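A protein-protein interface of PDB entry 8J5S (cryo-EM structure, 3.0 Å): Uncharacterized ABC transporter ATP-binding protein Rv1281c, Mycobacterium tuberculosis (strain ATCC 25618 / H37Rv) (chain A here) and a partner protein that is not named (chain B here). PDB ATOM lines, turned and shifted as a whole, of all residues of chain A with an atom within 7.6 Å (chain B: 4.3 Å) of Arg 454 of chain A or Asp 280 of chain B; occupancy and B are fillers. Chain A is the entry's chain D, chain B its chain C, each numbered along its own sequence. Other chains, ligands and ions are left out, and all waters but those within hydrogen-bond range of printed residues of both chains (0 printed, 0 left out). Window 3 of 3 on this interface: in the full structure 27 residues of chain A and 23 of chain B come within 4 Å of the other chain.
The side-chain amide oxygen of Asn 199 of chain B lies within hydrogen-bond range of the guanidinium group of Arg 454 of chain A (3.1 Å). OG of Ser 202 of chain B sits at hydrogen-bond distance from NH1 of Arg 454 of chain A, 3.4 Å away. NH1 of Arg 454 of chain A is in hydrogen-bond range of O of Leu 279 of chain B (3.4 Å). The side-chain carboxylate (OD2) of Asp 280 of chain B lies within salt-bridge range of the guanidinium group (NH2) of Arg 454 of chain A (3.4 Å).
O of Pro 198 of chain B is in hydrogen-bond range of OG of Ser 202 of chain B (3.0 Å). OG of Ser 202 of chain B sits at hydrogen-bond distance from O of Asn 199 of chain B (3.2 Å). OD1 of Asp 452 of chain A sits close to N of Arg 454 of chain A (3.3 Å).
Among the printed residues, merely in contact across the chains: Pro 456 of chain A with Arg 7 of chain B (3.5 Å), Leu 455 of chain A with Arg 7 of chain B (3.8 Å), Asp 459 of chain A with Arg 7 of chain B (3.9 Å), Arg 454 of chain A with Pro 198 of chain B (3.9 Å) and Arg 454 of chain A with Arg 7 of chain B (3.9 Å).
Of chain B, only Arg 7, Pro 198, Asn 199, Ser 202, Leu 279 and Asp 280 come within 4 Å of Arg 454 of chain A. Of the printed residues of chain B, Asp 459 of chain A touches Arg 7 (3.9 Å). Of the printed residues of chain A, Pro 198 of chain B touches Arg 454 (3.9 Å). Asp 280 of chain B touches just one residue of chain A: Arg 454. The nearest printed residue of chain B that does not touch Arg 454 of chain A is Pro 281 of chain B (6.4 Å). The nearest printed residue of chain A that does not touch Asp 280 of chain B is Tyr 496 of chain A (7.9 Å). The nearest printed residue of chain A that does not touch Asn 199 of chain B is Asp 452 of chain A (4.5 Å).
Of the 12 printed residues of chain B, 6 touch a printed residue of chain A. Hydrophobic or aromatic side chains of chain A within 4 Å of the printed part of chain B: Leu 455 and Pro 456. Among the printed residues, Asp or Glu carboxylates within 4 Å of a Lys or Arg side-chain nitrogen of the other chain: Arg 454 of chain A with Asp 280 of chain B (3.4 Å).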
ATOM      1  N   LEU A 451      11.365  -6.039  30.439  1.00  0.00           N
ATOM      2  CA  LEU A 451      12.740  -5.612  30.656  1.00  0.00           C
ATOM      3  C   LEU A 451      13.134  -4.616  29.579  1.00  0.00           C
ATOM      4  O   LEU A 451      12.936  -4.877  28.390  1.00  0.00           O
ATOM      5  CB  LEU A 451      13.692  -6.806  30.634  1.00  0.00           C
ATOM      6  CG  LEU A 451      13.464  -7.929  31.639  1.00  0.00           C
ATOM      7  CD1 LEU A 451      14.393  -9.076  31.347  1.00  0.00           C
ATOM      8  CD2 LEU A 451      13.683  -7.437  33.041  1.00  0.00           C
ATOM      9  N   ASP A 452      13.694  -3.488  29.991  1.00  0.00           N
ATOM     10  CA  ASP A 452      14.158  -2.483  29.048  1.00  0.00           C
ATOM     11  C   ASP A 452      15.296  -3.059  28.220  1.00  0.00           C
ATOM     12  O   ASP A 452      16.316  -3.468  28.787  1.00  0.00           O
ATOM     13  CB  ASP A 452      14.615  -1.238  29.803  1.00  0.00           C
ATOM     14  CG  ASP A 452      15.052  -0.106  28.888  1.00  0.00           C
ATOM     15  OD1 ASP A 452      15.050  -0.269  27.658  1.00  0.00           O
ATOM     16  OD2 ASP A 452      15.407   0.967  29.411  1.00  0.00           O
ATOM     17  N   PRO A 453      15.178  -3.104  26.891  1.00  0.00           N
ATOM     18  CA  PRO A 453      16.187  -3.798  26.085  1.00  0.00           C
ATOM     19  C   PRO A 453      17.506  -3.066  25.942  1.00  0.00           C
ATOM     20  O   PRO A 453      18.384  -3.570  25.236  1.00  0.00           O
ATOM     21  CB  PRO A 453      15.496  -3.945  24.726  1.00  0.00           C
ATOM     22  CG  PRO A 453      14.502  -2.862  24.690  1.00  0.00           C
ATOM     23  CD  PRO A 453      14.014  -2.708  26.087  1.00  0.00           C
ATOM     24  N   ARG A 454      17.697  -1.909  26.568  1.00  0.00           N
ATOM     25  CA  ARG A 454      18.969  -1.208  26.453  1.00  0.00           C
ATOM     26  C   ARG A 454      19.496  -0.797  27.824  1.00  0.00           C
ATOM     27  O   ARG A 454      20.131   0.243  27.991  1.00  0.00           O
ATOM     28  CB  ARG A 454      18.856  -0.030  25.485  1.00  0.00           C
ATOM     29  CG  ARG A 454      18.322   1.274  26.016  1.00  0.00           C
ATOM     30  CD  ARG A 454      18.717   2.401  25.082  1.00  0.00           C
ATOM     31  NE  ARG A 454      18.367   2.080  23.704  1.00  0.00           N
ATOM     32  CZ  ARG A 454      19.036   2.510  22.639  1.00  0.00           C
ATOM     33  NH1 ARG A 454      20.102   3.281  22.787  1.00  0.00           N
ATOM     34  NH2 ARG A 454      18.638   2.163  21.425  1.00  0.00           N
ATOM     35  N   LEU A 455      19.290  -1.652  28.818  1.00  0.00           N
ATOM     36  CA  LEU A 455      19.971  -1.531  30.091  1.00  0.00           C
ATOM     37  C   LEU A 455      20.648  -2.853  30.415  1.00  0.00           C
ATOM     38  O   LEU A 455      20.056  -3.914  30.207  1.00  0.00           O
ATOM     39  CB  LEU A 455      19.001  -1.166  31.220  1.00  0.00           C
ATOM     40  CG  LEU A 455      18.350   0.208  31.252  1.00  0.00           C
ATOM     41  CD1 LEU A 455      17.042   0.116  31.975  1.00  0.00           C
ATOM     42  CD2 LEU A 455      19.252   1.193  31.946  1.00  0.00           C
ATOM     43  N   PRO A 456      21.873  -2.831  30.919  1.00  0.00           N
ATOM     44  CA  PRO A 456      22.523  -4.073  31.338  1.00  0.00           C
ATOM     45  C   PRO A 456      21.818  -4.682  32.535  1.00  0.00           C
ATOM     46  O   PRO A 456      20.981  -4.060  33.185  1.00  0.00           O
ATOM     47  CB  PRO A 456      23.945  -3.636  31.686  1.00  0.00           C
ATOM     48  CG  PRO A 456      23.873  -2.197  31.890  1.00  0.00           C
ATOM     49  CD  PRO A 456      22.783  -1.687  31.014  1.00  0.00           C
ATOM     50  N   ASP A 459      21.777  -2.828  35.837  1.00  0.00           N
ATOM     51  CA  ASP A 459      20.854  -1.705  35.896  1.00  0.00           C
ATOM     52  C   ASP A 459      19.412  -2.175  36.007  1.00  0.00           C
ATOM     53  O   ASP A 459      18.603  -1.543  36.690  1.00  0.00           O
ATOM     54  CB  ASP A 459      21.038  -0.814  34.674  1.00  0.00           C
ATOM     55  CG  ASP A 459      22.265   0.066  34.779  1.00  0.00           C
ATOM     56  OD1 ASP A 459      22.138   1.210  35.263  1.00  0.00           O
ATOM     57  OD2 ASP A 459      23.361  -0.389  34.398  1.00  0.00           O
ATOM     58  N   LEU A 460      19.066  -3.274  35.338  1.00  0.00           N
ATOM     59  CA  LEU A 460      17.703  -3.782  35.409  1.00  0.00           C
ATOM     60  C   LEU A 460      17.375  -4.277  36.809  1.00  0.00           C
ATOM     61  O   LEU A 460      16.351  -3.903  37.385  1.00  0.00           O
ATOM     62  CB  LEU A 460      17.506  -4.905  34.397  1.00  0.00           C
ATOM     63  CG  LEU A 460      17.521  -4.541  32.923  1.00  0.00           C
ATOM     64  CD1 LEU A 460      17.481  -5.797  32.107  1.00  0.00           C
ATOM     65  CD2 LEU A 460      16.348  -3.666  32.600  1.00  0.00           C
ATOM     66  N   TYR A 496      23.527  -7.378  28.056  1.00  0.00           N
ATOM     67  CA  TYR A 496      22.227  -6.803  27.770  1.00  0.00           C
ATOM     68  C   TYR A 496      21.157  -7.889  27.720  1.00  0.00           C
ATOM     69  O   TYR A 496      21.465  -9.067  27.544  1.00  0.00           O
ATOM     70  CB  TYR A 496      22.291  -6.037  26.457  1.00  0.00           C
ATOM     71  CG  TYR A 496      22.757  -4.616  26.639  1.00  0.00           C
ATOM     72  CD1 TYR A 496      24.099  -4.319  26.775  1.00  0.00           C
ATOM     73  CD2 TYR A 496      21.855  -3.578  26.689  1.00  0.00           C
ATOM     74  CE1 TYR A 496      24.524  -3.024  26.952  1.00  0.00           C
ATOM     75  CE2 TYR A 496      22.272  -2.282  26.863  1.00  0.00           C
ATOM     76  CZ  TYR A 496      23.605  -2.008  26.995  1.00  0.00           C
ATOM     77  OH  TYR A 496      24.015  -0.706  27.171  1.00  0.00           O
ATOM     78  N   PRO A 497      19.883  -7.523  27.897  1.00  0.00           N
ATOM     79  CA  PRO A 497      18.831  -8.549  27.910  1.00  0.00           C
ATOM     80  C   PRO A 497      18.728  -9.332  26.621  1.00  0.00           C
ATOM     81  O   PRO A 497      18.375 -10.514  26.657  1.00  0.00           O
ATOM     82  CB  PRO A 497      17.554  -7.740  28.167  1.00  0.00           C
ATOM     83  CG  PRO A 497      18.002  -6.454  28.697  1.00  0.00           C
ATOM     84  CD  PRO A 497      19.328  -6.179  28.101  1.00  0.00           C
ATOM     85  N   ALA A 498      19.018  -8.710  25.481  1.00  0.00           N
ATOM     86  CA  ALA A 498      18.804  -9.365  24.198  1.00  0.00           C
ATOM     87  C   ALA A 498      19.735 -10.546  23.975  1.00  0.00           C
ATOM     88  O   ALA A 498      19.425 -11.407  23.149  1.00  0.00           O
ATOM     89  CB  ALA A 498      18.963  -8.359  23.062  1.00  0.00           C
ATOM     90  N   ARG B   7      26.823   2.032  33.101  1.00  0.00           N
ATOM     91  CA  ARG B   7      26.291   1.931  31.749  1.00  0.00           C
ATOM     92  C   ARG B   7      26.915   2.930  30.790  1.00  0.00           C
ATOM     93  O   ARG B   7      27.188   2.584  29.638  1.00  0.00           O
ATOM     94  CB  ARG B   7      24.776   2.126  31.757  1.00  0.00           C
ATOM     95  CG  ARG B   7      24.085   1.499  30.578  1.00  0.00           C
ATOM     96  CD  ARG B   7      22.645   1.943  30.493  1.00  0.00           C
ATOM     97  NE  ARG B   7      22.501   3.359  30.800  1.00  0.00           N
ATOM     98  CZ  ARG B   7      22.176   4.284  29.904  1.00  0.00           C
ATOM     99  NH1 ARG B   7      21.960   3.939  28.645  1.00  0.00           N
ATOM    100  NH2 ARG B   7      22.066   5.552  30.267  1.00  0.00           N
ATOM    101  N   PRO B 198      17.714   8.182  27.689  1.00  0.00           N
ATOM    102  CA  PRO B 198      18.718   7.292  27.098  1.00  0.00           C
ATOM    103  C   PRO B 198      18.333   6.776  25.730  1.00  0.00           C
ATOM    104  O   PRO B 198      19.212   6.432  24.937  1.00  0.00           O
ATOM    105  CB  PRO B 198      18.816   6.156  28.120  1.00  0.00           C
ATOM    106  CG  PRO B 198      18.451   6.787  29.387  1.00  0.00           C
ATOM    107  CD  PRO B 198      17.360   7.745  29.047  1.00  0.00           C
ATOM    108  N   ASN B 199      17.042   6.702  25.425  1.00  0.00           N
ATOM    109  CA  ASN B 199      16.637   6.249  24.103  1.00  0.00           C
ATOM    110  C   ASN B 199      16.706   7.383  23.090  1.00  0.00           C
ATOM    111  O   ASN B 199      17.465   7.311  22.120  1.00  0.00           O
ATOM    112  CB  ASN B 199      15.236   5.642  24.163  1.00  0.00           C
ATOM    113  CG  ASN B 199      15.266   4.138  24.294  1.00  0.00           C
ATOM    114  OD1 ASN B 199      15.577   3.429  23.339  1.00  0.00           O
ATOM    115  ND2 ASN B 199      14.959   3.640  25.487  1.00  0.00           N
ATOM    116  N   SER B 202      20.452   9.353  22.155  1.00  0.00           N
ATOM    117  CA  SER B 202      21.471   8.672  21.381  1.00  0.00           C
ATOM    118  C   SER B 202      21.071   8.493  19.937  1.00  0.00           C
ATOM    119  O   SER B 202      21.934   8.500  19.059  1.00  0.00           O
ATOM    120  CB  SER B 202      21.770   7.301  21.989  1.00  0.00           C
ATOM    121  OG  SER B 202      20.570   6.625  22.299  1.00  0.00           O
ATOM    122  N   ARG B 276      26.266   4.403  15.428  1.00  0.00           N
ATOM    123  CA  ARG B 276      25.055   3.589  15.413  1.00  0.00           C
ATOM    124  C   ARG B 276      25.333   2.182  15.916  1.00  0.00           C
ATOM    125  O   ARG B 276      24.521   1.605  16.646  1.00  0.00           O
ATOM    126  CB  ARG B 276      24.469   3.540  14.007  1.00  0.00           C
ATOM    127  CG  ARG B 276      23.056   3.011  13.952  1.00  0.00           C
ATOM    128  CD  ARG B 276      22.542   2.966  12.526  1.00  0.00           C
ATOM    129  NE  ARG B 276      21.691   4.109  12.212  1.00  0.00           N
ATOM    130  CZ  ARG B 276      22.033   5.086  11.378  1.00  0.00           C
ATOM    131  NH1 ARG B 276      23.211   5.064  10.774  1.00  0.00           N
ATOM    132  NH2 ARG B 276      21.195   6.086  11.148  1.00  0.00           N
ATOM    133  N   ASP B 277      26.471   1.607  15.534  1.00  0.00           N
ATOM    134  CA  ASP B 277      26.806   0.265  15.992  1.00  0.00           C
ATOM    135  C   ASP B 277      27.202   0.230  17.458  1.00  0.00           C
ATOM    136  O   ASP B 277      27.079  -0.819  18.091  1.00  0.00           O
ATOM    137  CB  ASP B 277      27.932  -0.322  15.147  1.00  0.00           C
ATOM    138  CG  ASP B 277      27.419  -1.223  14.044  1.00  0.00           C
ATOM    139  OD1 ASP B 277      26.221  -1.574  14.072  1.00  0.00           O
ATOM    140  OD2 ASP B 277      28.215  -1.581  13.150  1.00  0.00           O
ATOM    141  N   ALA B 278      27.689   1.337  18.008  1.00  0.00           N
ATOM    142  CA  ALA B 278      28.072   1.371  19.412  1.00  0.00           C
ATOM    143  C   ALA B 278      26.899   1.659  20.336  1.00  0.00           C
ATOM    144  O   ALA B 278      26.834   1.104  21.435  1.00  0.00           O
ATOM    145  CB  ALA B 278      29.167   2.413  19.634  1.00  0.00           C
ATOM    146  N   LEU B 279      25.974   2.521  19.925  1.00  0.00           N
ATOM    147  CA  LEU B 279      24.803   2.813  20.744  1.00  0.00           C
ATOM    148  C   LEU B 279      23.675   1.811  20.550  1.00  0.00           C
ATOM    149  O   LEU B 279      22.795   1.720  21.411  1.00  0.00           O
ATOM    150  CB  LEU B 279      24.289   4.221  20.453  1.00  0.00           C
ATOM    151  CG  LEU B 279      25.221   5.332  20.925  1.00  0.00           C
ATOM    152  CD1 LEU B 279      25.040   6.576  20.092  1.00  0.00           C
ATOM    153  CD2 LEU B 279      24.986   5.636  22.385  1.00  0.00           C
ATOM    154  N   ASP B 280      23.680   1.063  19.448  1.00  0.00           N
ATOM    155  CA  ASP B 280      22.716  -0.007  19.191  1.00  0.00           C
ATOM    156  C   ASP B 280      23.496  -1.271  18.857  1.00  0.00           C
ATOM    157  O   ASP B 280      23.543  -1.696  17.697  1.00  0.00           O
ATOM    158  CB  ASP B 280      21.765   0.359  18.053  1.00  0.00           C
ATOM    159  CG  ASP B 280      20.837   1.504  18.404  1.00  0.00           C
ATOM    160  OD1 ASP B 280      19.726   1.560  17.843  1.00  0.00           O
ATOM    161  OD2 ASP B 280      21.215   2.356  19.231  1.00  0.00           O
ATOM    162  N   PRO B 281      24.116  -1.904  19.862  1.00  0.00           N
ATOM    163  CA  PRO B 281      25.159  -2.901  19.586  1.00  0.00           C
ATOM    164  C   PRO B 281      24.782  -4.017  18.624  1.00  0.00           C
ATOM    165  O   PRO B 281      25.367  -4.129  17.541  1.00  0.00           O
ATOM    166  CB  PRO B 281      25.446  -3.473  20.978  1.00  0.00           C
ATOM    167  CG  PRO B 281      25.207  -2.337  21.889  1.00  0.00           C
ATOM    168  CD  PRO B 281      24.041  -1.582  21.298  1.00  0.00           C
ATOM    169  N   ALA B 282      23.815  -4.843  18.997  1.00  0.00           N
ATOM    170  CA  ALA B 282      23.289  -5.868  18.099  1.00  0.00           C
ATOM    171  C   ALA B 282      21.973  -5.404  17.479  1.00  0.00           C
ATOM    172  O   ALA B 282      20.939  -6.065  17.581  1.00  0.00           O
ATOM    173  CB  ALA B 282      23.125  -7.189  18.843  1.00  0.00           C
ATOM    174  N   SER B 283      22.037  -4.245  16.828  1.00  0.00           N
ATOM    175  CA  SER B 283      20.879  -3.647  16.171  1.00  0.00           C
ATOM    176  C   SER B 283      19.682  -3.533  17.109  1.00  0.00           C
ATOM    177  O   SER B 283      18.709  -4.278  16.979  1.00  0.00           O
ATOM    178  CB  SER B 283      20.498  -4.456  14.933  1.00  0.00           C
ATOM    179  OG  SER B 283      19.836  -5.653  15.296  1.00  0.00           O
